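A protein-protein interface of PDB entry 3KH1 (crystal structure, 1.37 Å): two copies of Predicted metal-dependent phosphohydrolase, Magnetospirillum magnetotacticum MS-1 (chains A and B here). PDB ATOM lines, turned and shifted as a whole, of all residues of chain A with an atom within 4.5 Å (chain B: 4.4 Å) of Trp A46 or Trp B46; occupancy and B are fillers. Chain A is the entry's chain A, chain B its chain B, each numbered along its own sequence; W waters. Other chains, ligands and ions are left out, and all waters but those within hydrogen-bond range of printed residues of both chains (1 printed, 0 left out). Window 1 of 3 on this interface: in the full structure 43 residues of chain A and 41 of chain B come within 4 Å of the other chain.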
ATOM      1  N   ILE A  20      29.535   5.095 -19.908  1.00  0.00           N
ATOM      2  CA  ILE A  20      28.839   4.233 -18.957  1.00  0.00           C
ATOM      3  C   ILE A  20      27.420   3.918 -19.381  1.00  0.00           C
ATOM      4  O   ILE A  20      26.789   3.078 -18.728  1.00  0.00           O
ATOM      5  CB  ILE A  20      28.958   4.755 -17.491  1.00  0.00           C
ATOM      6  CG1 ILE A  20      28.210   6.065 -17.274  1.00  0.00           C
ATOM      7  CG2 ILE A  20      30.419   4.828 -17.032  1.00  0.00           C
ATOM      8  CD1 ILE A  20      28.165   6.551 -15.782  1.00  0.00           C
ATOM      9  N   LEU A  23      26.743   0.165 -19.421  1.00  0.00           N
ATOM     10  CA  LEU A  23      26.363  -0.697 -18.282  1.00  0.00           C
ATOM     11  C   LEU A  23      24.975  -1.287 -18.491  1.00  0.00           C
ATOM     12  O   LEU A  23      24.625  -2.344 -17.961  1.00  0.00           O
ATOM     13  CB  LEU A  23      26.460   0.078 -16.969  1.00  0.00           C
ATOM     14  CG  LEU A  23      26.265  -0.765 -15.708  1.00  0.00           C
ATOM     15  CD1 LEU A  23      27.394  -1.807 -15.624  1.00  0.00           C
ATOM     16  CD2 LEU A  23      26.211   0.123 -14.513  1.00  0.00           C
ATOM     17  N   LYS A  24      24.160  -0.575 -19.255  1.00  0.00           N
ATOM     18  CA  LYS A  24      22.777  -0.968 -19.535  1.00  0.00           C
ATOM     19  C   LYS A  24      22.686  -2.277 -20.312  1.00  0.00           C
ATOM     20  O   LYS A  24      21.627  -2.908 -20.254  1.00  0.00           O
ATOM     21  CB  LYS A  24      22.075   0.166 -20.306  1.00  0.00           C
ATOM     22  CG  LYS A  24      21.954   1.466 -19.463  1.00  0.00           C
ATOM     23  CD  LYS A  24      21.568   2.676 -20.295  1.00  0.00           C
ATOM     24  CE  LYS A  24      21.689   3.965 -19.498  1.00  0.00           C
ATOM     25  NZ  LYS A  24      21.424   5.188 -20.351  1.00  0.00           N
ATOM     26  N   ALA A  42      22.559  -1.623 -14.926  1.00  0.00           N
ATOM     27  CA  ALA A  42      22.194  -0.212 -14.678  1.00  0.00           C
ATOM     28  C   ALA A  42      20.894  -0.159 -13.897  1.00  0.00           C
ATOM     29  O   ALA A  42      20.788   0.567 -12.912  1.00  0.00           O
ATOM     30  CB  ALA A  42      22.083   0.568 -16.003  1.00  0.00           C
ATOM     31  N   GLU A  43      19.881  -0.911 -14.320  1.00  0.00           N
ATOM     32  CA  GLU A  43      18.593  -0.849 -13.606  1.00  0.00           C
ATOM     33  C   GLU A  43      18.712  -1.511 -12.228  1.00  0.00           C
ATOM     34  O   GLU A  43      18.054  -1.073 -11.302  1.00  0.00           O
ATOM     35  CB  GLU A  43      17.487  -1.387 -14.407  1.00  0.00           C
ATOM     36  CG  GLU A  43      17.605  -2.771 -14.642  1.00  0.00           C
ATOM     37  CD  GLU A  43      16.672  -3.326 -15.848  1.00  0.00           C
ATOM     38  OE1 GLU A  43      15.918  -2.613 -16.551  1.00  0.00           O
ATOM     39  OE2 GLU A  43      16.788  -4.485 -16.044  1.00  0.00           O
ATOM     40  N   HIS A  44      19.631  -2.471 -12.056  1.00  0.00           N
ATOM     41  CA  HIS A  44      19.918  -3.049 -10.732  1.00  0.00           C
ATOM     42  C   HIS A  44      20.491  -1.988  -9.811  1.00  0.00           C
ATOM     43  O   HIS A  44      20.010  -1.848  -8.671  1.00  0.00           O
ATOM     44  CB  HIS A  44      20.895  -4.231 -10.863  1.00  0.00           C
ATOM     45  CG  HIS A  44      21.258  -4.859  -9.559  1.00  0.00           C
ATOM     46  ND1 HIS A  44      20.416  -5.748  -8.912  1.00  0.00           N
ATOM     47  CD2 HIS A  44      22.318  -4.671  -8.730  1.00  0.00           C
ATOM     48  CE1 HIS A  44      20.996  -6.140  -7.787  1.00  0.00           C
ATOM     49  NE2 HIS A  44      22.116  -5.467  -7.630  1.00  0.00           N
ATOM     50  N   SER A  45      21.486  -1.227 -10.295  1.00  0.00           N
ATOM     51  CA  SER A  45      22.091  -0.189  -9.478  1.00  0.00           C
ATOM     52  C   SER A  45      21.046   0.911  -9.170  1.00  0.00           C
ATOM     53  O   SER A  45      21.055   1.446  -8.053  1.00  0.00           O
ATOM     54  CB  SER A  45      23.343   0.373 -10.129  1.00  0.00           C
ATOM     55  OG  SER A  45      24.417  -0.549  -9.968  1.00  0.00           O
ATOM     56  N   TRP A  46      20.197   1.297 -10.131  1.00  0.00           N
ATOM     57  CA  TRP A  46      19.086   2.201  -9.812  1.00  0.00           C
ATOM     58  C   TRP A  46      18.309   1.680  -8.611  1.00  0.00           C
ATOM     59  O   TRP A  46      18.011   2.427  -7.679  1.00  0.00           O
ATOM     60  CB  TRP A  46      18.124   2.339 -11.024  1.00  0.00           C
ATOM     61  CG  TRP A  46      16.834   3.002 -10.612  1.00  0.00           C
ATOM     62  CD1 TRP A  46      16.653   4.316 -10.425  1.00  0.00           C
ATOM     63  CD2 TRP A  46      15.604   2.352 -10.311  1.00  0.00           C
ATOM     64  NE1 TRP A  46      15.404   4.563  -9.984  1.00  0.00           N
ATOM     65  CE2 TRP A  46      14.722   3.359  -9.911  1.00  0.00           C
ATOM     66  CE3 TRP A  46      15.182   1.032 -10.345  1.00  0.00           C
ATOM     67  CZ2 TRP A  46      13.425   3.099  -9.498  1.00  0.00           C
ATOM     68  CZ3 TRP A  46      13.852   0.767  -9.978  1.00  0.00           C
ATOM     69  CH2 TRP A  46      12.998   1.796  -9.550  1.00  0.00           C
ATOM     70  N   HIS A  47      17.941   0.426  -8.653  1.00  0.00           N
ATOM     71  CA  HIS A  47      17.053  -0.125  -7.663  1.00  0.00           C
ATOM     72  C   HIS A  47      17.664  -0.151  -6.293  1.00  0.00           C
ATOM     73  O   HIS A  47      17.050   0.281  -5.314  1.00  0.00           O
ATOM     74  CB  HIS A  47      16.665  -1.537  -8.097  1.00  0.00           C
ATOM     75  CG  HIS A  47      15.357  -2.032  -7.554  1.00  0.00           C
ATOM     76  ND1 HIS A  47      14.855  -3.259  -7.911  1.00  0.00           N
ATOM     77  CD2 HIS A  47      14.466  -1.492  -6.685  1.00  0.00           C
ATOM     78  CE1 HIS A  47      13.682  -3.432  -7.316  1.00  0.00           C
ATOM     79  NE2 HIS A  47      13.406  -2.374  -6.582  1.00  0.00           N
ATOM     80  N   ILE A  48      18.922  -0.570  -6.201  1.00  0.00           N
ATOM     81  CA  ILE A  48      19.574  -0.657  -4.885  1.00  0.00           C
ATOM     82  C   ILE A  48      19.895   0.722  -4.331  1.00  0.00           C
ATOM     83  O   ILE A  48      19.841   0.936  -3.140  1.00  0.00           O
ATOM     84  CB  ILE A  48      20.925  -1.431  -4.878  1.00  0.00           C
ATOM     85  CG1 ILE A  48      20.953  -2.692  -5.754  1.00  0.00           C
ATOM     86  CG2 ILE A  48      21.296  -1.820  -3.432  1.00  0.00           C
ATOM     87  CD1 ILE A  48      19.721  -3.602  -5.578  1.00  0.00           C
ATOM     88  N   ALA A  49      20.305   1.658  -5.195  1.00  0.00           N
ATOM     89  CA  ALA A  49      20.538   3.025  -4.703  1.00  0.00           C
ATOM     90  C   ALA A  49      19.262   3.663  -4.179  1.00  0.00           C
ATOM     91  O   ALA A  49      19.293   4.360  -3.160  1.00  0.00           O
ATOM     92  CB  ALA A  49      21.175   3.901  -5.807  1.00  0.00           C
ATOM     93  N   THR A  50      18.135   3.405  -4.833  1.00  0.00           N
ATOM     94  CA  THR A  50      16.874   3.906  -4.337  1.00  0.00           C
ATOM     95  C   THR A  50      16.530   3.249  -2.979  1.00  0.00           C
ATOM     96  O   THR A  50      16.099   3.923  -2.038  1.00  0.00           O
ATOM     97  CB  THR A  50      15.760   3.643  -5.383  1.00  0.00           C
ATOM     98  OG1 THR A  50      16.131   4.250  -6.622  1.00  0.00           O
ATOM     99  CG2 THR A  50      14.425   4.207  -4.950  1.00  0.00           C
ATOM    100  N   LEU A  73      25.688   3.336  -7.116  1.00  0.00           N
ATOM    101  CA  LEU A  73      25.531   3.768  -8.513  1.00  0.00           C
ATOM    102  C   LEU A  73      26.764   3.365  -9.333  1.00  0.00           C
ATOM    103  O   LEU A  73      26.646   3.064 -10.513  1.00  0.00           O
ATOM    104  CB  LEU A  73      25.311   5.248  -8.629  1.00  0.00           C
ATOM    105  CG  LEU A  73      23.965   5.732  -8.034  1.00  0.00           C
ATOM    106  CD1 LEU A  73      23.941   7.266  -7.994  1.00  0.00           C
ATOM    107  CD2 LEU A  73      22.772   5.216  -8.895  1.00  0.00           C
ATOM    108  N   ILE B  20       8.168  -0.854  -7.433  1.00  0.00           N
ATOM    109  CA  ILE B  20       8.948   0.026  -8.299  1.00  0.00           C
ATOM    110  C   ILE B  20       9.864  -0.693  -9.262  1.00  0.00           C
ATOM    111  O   ILE B  20      10.392  -0.103 -10.211  1.00  0.00           O
ATOM    112  CB  ILE B  20       9.670   1.171  -7.567  1.00  0.00           C
ATOM    113  CG1 ILE B  20      10.817   0.669  -6.688  1.00  0.00           C
ATOM    114  CG2 ILE B  20       8.613   2.024  -6.776  1.00  0.00           C
ATOM    115  CD1 ILE B  20      11.631   1.750  -6.029  1.00  0.00           C
ATOM    116  N   LEU B  23       9.300   0.103 -12.887  1.00  0.00           N
ATOM    117  CA  LEU B  23       9.858   1.233 -13.638  1.00  0.00           C
ATOM    118  C   LEU B  23      10.789   0.752 -14.759  1.00  0.00           C
ATOM    119  O   LEU B  23      10.972   1.392 -15.784  1.00  0.00           O
ATOM    120  CB  LEU B  23      10.577   2.201 -12.683  1.00  0.00           C
ATOM    121  CG  LEU B  23      10.990   3.516 -13.357  1.00  0.00           C
ATOM    122  CD1 LEU B  23       9.766   4.289 -13.916  1.00  0.00           C
ATOM    123  CD2 LEU B  23      11.817   4.349 -12.389  1.00  0.00           C
ATOM    124  N   LYS B  24      11.395  -0.412 -14.542  1.00  0.00           N
ATOM    125  CA  LYS B  24      12.277  -1.033 -15.525  1.00  0.00           C
ATOM    126  C   LYS B  24      11.568  -1.426 -16.821  1.00  0.00           C
ATOM    127  O   LYS B  24      12.246  -1.686 -17.825  1.00  0.00           O
ATOM    128  CB  LYS B  24      12.942  -2.267 -14.900  1.00  0.00           C
ATOM    129  CG  LYS B  24      13.793  -1.935 -13.664  1.00  0.00           C
ATOM    130  CD  LYS B  24      14.223  -3.173 -12.888  1.00  0.00           C
ATOM    131  CE  LYS B  24      14.802  -2.865 -11.532  1.00  0.00           C
ATOM    132  NZ  LYS B  24      14.968  -4.077 -10.692  1.00  0.00           N
ATOM    133  N   ALA B  42      14.117   3.225 -15.570  1.00  0.00           N
ATOM    134  CA  ALA B  42      14.936   2.910 -14.430  1.00  0.00           C
ATOM    135  C   ALA B  42      16.391   3.098 -14.754  1.00  0.00           C
ATOM    136  O   ALA B  42      17.129   3.780 -14.014  1.00  0.00           O
ATOM    137  CB  ALA B  42      14.665   1.492 -13.916  1.00  0.00           C
ATOM    138  N   GLU B  43      16.893   2.545 -15.851  1.00  0.00           N
ATOM    139  CA  GLU B  43      18.283   2.698 -16.185  1.00  0.00           C
ATOM    140  C   GLU B  43      18.588   4.163 -16.544  1.00  0.00           C
ATOM    141  O   GLU B  43      19.702   4.649 -16.317  1.00  0.00           O
ATOM    142  CB  GLU B  43      18.681   1.746 -17.282  1.00  0.00           C
ATOM    143  CG  GLU B  43      18.014   2.006 -18.622  1.00  0.00           C
ATOM    144  CD  GLU B  43      18.105   0.869 -19.613  1.00  0.00           C
ATOM    145  OE1 GLU B  43      18.771  -0.138 -19.317  1.00  0.00           O
ATOM    146  OE2 GLU B  43      17.521   1.004 -20.694  1.00  0.00           O
ATOM    147  N   HIS B  44      17.615   4.903 -17.075  1.00  0.00           N
ATOM    148  CA  HIS B  44      17.807   6.311 -17.336  1.00  0.00           C
ATOM    149  C   HIS B  44      18.012   7.080 -16.030  1.00  0.00           C
ATOM    150  O   HIS B  44      18.932   7.926 -15.928  1.00  0.00           O
ATOM    151  CB  HIS B  44      16.602   6.900 -18.087  1.00  0.00           C
ATOM    152  CG  HIS B  44      16.766   8.339 -18.440  1.00  0.00           C
ATOM    153  ND1 HIS B  44      17.662   8.757 -19.385  1.00  0.00           N
ATOM    154  CD2 HIS B  44      16.175   9.451 -17.950  1.00  0.00           C
ATOM    155  CE1 HIS B  44      17.614  10.076 -19.462  1.00  0.00           C
ATOM    156  NE2 HIS B  44      16.724  10.524 -18.586  1.00  0.00           N
ATOM    157  N   SER B  45      17.203   6.754 -15.008  1.00  0.00           N
ATOM    158  CA  SER B  45      17.376   7.401 -13.701  1.00  0.00           C
ATOM    159  C   SER B  45      18.683   7.026 -13.030  1.00  0.00           C
ATOM    160  O   SER B  45      19.299   7.889 -12.425  1.00  0.00           O
ATOM    161  CB  SER B  45      16.176   7.108 -12.804  1.00  0.00           C
ATOM    162  OG  SER B  45      15.042   7.894 -13.176  1.00  0.00           O
ATOM    163  N   TRP B  46      19.148   5.788 -13.165  1.00  0.00           N
ATOM    164  CA  TRP B  46      20.467   5.425 -12.727  1.00  0.00           C
ATOM    165  C   TRP B  46      21.522   6.387 -13.354  1.00  0.00           C
ATOM    166  O   TRP B  46      22.403   6.930 -12.675  1.00  0.00           O
ATOM    167  CB  TRP B  46      20.851   3.992 -13.201  1.00  0.00           C
ATOM    168  CG  TRP B  46      22.324   3.724 -13.105  1.00  0.00           C
ATOM    169  CD1 TRP B  46      23.052   3.457 -11.979  1.00  0.00           C
ATOM    170  CD2 TRP B  46      23.277   3.789 -14.186  1.00  0.00           C
ATOM    171  NE1 TRP B  46      24.389   3.367 -12.291  1.00  0.00           N
ATOM    172  CE2 TRP B  46      24.540   3.591 -13.625  1.00  0.00           C
ATOM    173  CE3 TRP B  46      23.174   4.018 -15.583  1.00  0.00           C
ATOM    174  CZ2 TRP B  46      25.702   3.567 -14.392  1.00  0.00           C
ATOM    175  CZ3 TRP B  46      24.331   4.007 -16.333  1.00  0.00           C
ATOM    176  CH2 TRP B  46      25.559   3.771 -15.733  1.00  0.00           C
ATOM    177  N   HIS B  47      21.381   6.625 -14.653  1.00  0.00           N
ATOM    178  CA  HIS B  47      22.401   7.363 -15.381  1.00  0.00           C
ATOM    179  C   HIS B  47      22.439   8.807 -14.880  1.00  0.00           C
ATOM    180  O   HIS B  47      23.508   9.376 -14.659  1.00  0.00           O
ATOM    181  CB  HIS B  47      22.088   7.323 -16.891  1.00  0.00           C
ATOM    182  CG  HIS B  47      23.263   7.523 -17.798  1.00  0.00           C
ATOM    183  ND1 HIS B  47      23.206   7.151 -19.125  1.00  0.00           N
ATOM    184  CD2 HIS B  47      24.522   7.969 -17.584  1.00  0.00           C
ATOM    185  CE1 HIS B  47      24.378   7.399 -19.686  1.00  0.00           C
ATOM    186  NE2 HIS B  47      25.184   7.922 -18.788  1.00  0.00           N
ATOM    187  N   ILE B  48      21.268   9.430 -14.734  1.00  0.00           N
ATOM    188  CA  ILE B  48      21.182  10.841 -14.313  1.00  0.00           C
ATOM    189  C   ILE B  48      21.645  11.030 -12.879  1.00  0.00           C
ATOM    190  O   ILE B  48      22.373  11.991 -12.546  1.00  0.00           O
ATOM    191  CB  ILE B  48      19.801  11.523 -14.518  1.00  0.00           C
ATOM    192  CG1 ILE B  48      19.145  11.057 -15.813  1.00  0.00           C
ATOM    193  CG2 ILE B  48      20.001  13.046 -14.531  1.00  0.00           C
ATOM    194  CD1 ILE B  48      19.978  11.246 -17.049  1.00  0.00           C
ATOM    195  N   ALA B  49      21.256  10.095 -12.002  1.00  0.00           N
ATOM    196  CA  ALA B  49      21.690  10.146 -10.608  1.00  0.00           C
ATOM    197  C   ALA B  49      23.196  10.044 -10.509  1.00  0.00           C
ATOM    198  O   ALA B  49      23.802  10.722  -9.677  1.00  0.00           O
ATOM    199  CB  ALA B  49      20.983   9.100  -9.743  1.00  0.00           C
ATOM    200  N   THR B  50      23.798   9.189 -11.304  1.00  0.00           N
ATOM    201  CA  THR B  50      25.251   9.047 -11.319  1.00  0.00           C
ATOM    202  C   THR B  50      25.918  10.372 -11.750  1.00  0.00           C
ATOM    203  O   THR B  50      26.882  10.820 -11.147  1.00  0.00           O
ATOM    204  CB  THR B  50      25.671   7.866 -12.209  1.00  0.00           C
ATOM    205  OG1 THR B  50      25.056   6.665 -11.733  1.00  0.00           O
ATOM    206  CG2 THR B  50      27.181   7.664 -12.180  1.00  0.00           C
ATOM    207  N   LEU B  73      16.504   9.569  -8.608  1.00  0.00           N
ATOM    208  CA  LEU B  73      16.127   8.162  -8.543  1.00  0.00           C
ATOM    209  C   LEU B  73      14.628   7.955  -8.509  1.00  0.00           C
ATOM    210  O   LEU B  73      14.133   6.984  -9.060  1.00  0.00           O
ATOM    211  CB  LEU B  73      16.774   7.474  -7.358  1.00  0.00           C
ATOM    212  CG  LEU B  73      18.292   7.376  -7.408  1.00  0.00           C
ATOM    213  CD1 LEU B  73      18.834   6.928  -6.048  1.00  0.00           C
ATOM    214  CD2 LEU B  73      18.737   6.438  -8.506  1.00  0.00           C
HETATM  215  O   HOH W   1      20.380   7.987 -19.809  1.00  0.00           O
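The backbone carbonyl oxygen (O) of Trp A46 is in hydrogen-bond range of the side-chain hydroxyl (OG1) of Thr A50, at 2.8 Å.
The backbone carbonyl oxygen (O) of Trp B46 sits at hydrogen-bond distance from the side-chain hydroxyl (OG1) of Thr B50, at 2.8 Å.
Water W1 lies within hydrogen-bond range of a ring nitrogen (ND1) of His B44 (2.9 Å), a ring nitrogen (ND1) of His B47 (3.0 Å) and the side-chain amino group of Lys A24 (3.0 Å).
Among the printed residues, merely in contact across the chains: Ile A20 with Trp B46, Ile A20 with His B47, Ile A20 with Thr B50, Leu A23 with Trp B46, Lys A24 with Glu B43, Ala A42 with Glu B43, Ala A42 with Trp B46, Glu A43 with Lys B24, Ser A45 with Trp B46, Trp A46 with Ile B20, Trp A46 with Leu B23, Trp A46 with Ala B42, Trp A46 with Ser B45, Trp A46 with Trp B46, His A47 with Ile B20, Ala A49 with Leu B73, Thr A50 with Ile B20, Thr A50 with Leu B73, Leu A73 with Ala B49 and Leu A73 with Thr B50.
A ring nitrogen (ND1) of His B47 lies within hydrogen-bond range of the side-chain amino group (NZ) of Lys A24 (2.9 Å).
The backbone carbonyl oxygen of Leu B73 lies within hydrogen-bond range of the indole nitrogen of Trp A46, 2.9 Å away.
A ring nitrogen (ND1) of His A47 lies within hydrogen-bond range of the side-chain amino group (NZ) of Lys B24 (2.9 Å).
O of Leu A73 sits at hydrogen-bond distance from NE1 of Trp B46 (2.9 Å).
Along chain B the printed residues that touch a printed residue of chain A span positions 20 to 73.
Along chain A the printed residues that touch a printed residue of chain B span positions 20 to 73.
Among the printed residues, no Asp or Glu carboxylate lies within 4 Å of a Lys or Arg side-chain nitrogen of the other chain.
Trp A46 touches just these residues of chain B: Ile B20, Leu B23, Ala B42, Ser B45, Trp B46 and Leu B73.
Of chain A, only Ile A20 (3.3 Å), Leu A23 (3.5 Å), Ala A42 (3.4 Å), Ser A45 (3.6 Å), Trp A46 (3.9 Å) and Leu A73 (2.9 Å) come within 4 Å of Trp B46.
Printed residues of chain A within 4 Å of Ser B45: Trp A46 (3.7 Å).
Of the printed residues of chain A, Glu B43 touches Lys A24 (3.5 Å) and Ala A42 (3.8 Å).
Of the printed residues of chain A, Ile B20 touches Trp A46, His A47 and Thr A50.
Ile B48 touches none of the printed residues of chain A.
Ile A48 touches none of the printed residues of chain B.
The nearest residue of chain B that does not touch Trp A46 is Lys B24 (4.1 Å).
The nearest printed residue of chain A that does not touch Ala B42 is Glu A43 (4.1 Å).
Lys A24 touches Glu B43, and with the chains exchanged Glu A43 touches Lys B24.
Ser A45 touches Trp B46, and with the chains exchanged Trp A46 touches Ser B45.
Trp A46 touches Leu B73, and with the chains exchanged Leu A73 touches Trp B46.
Ala A49 touches Leu B73, and with the chains exchanged Leu A73 touches Ala B49.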
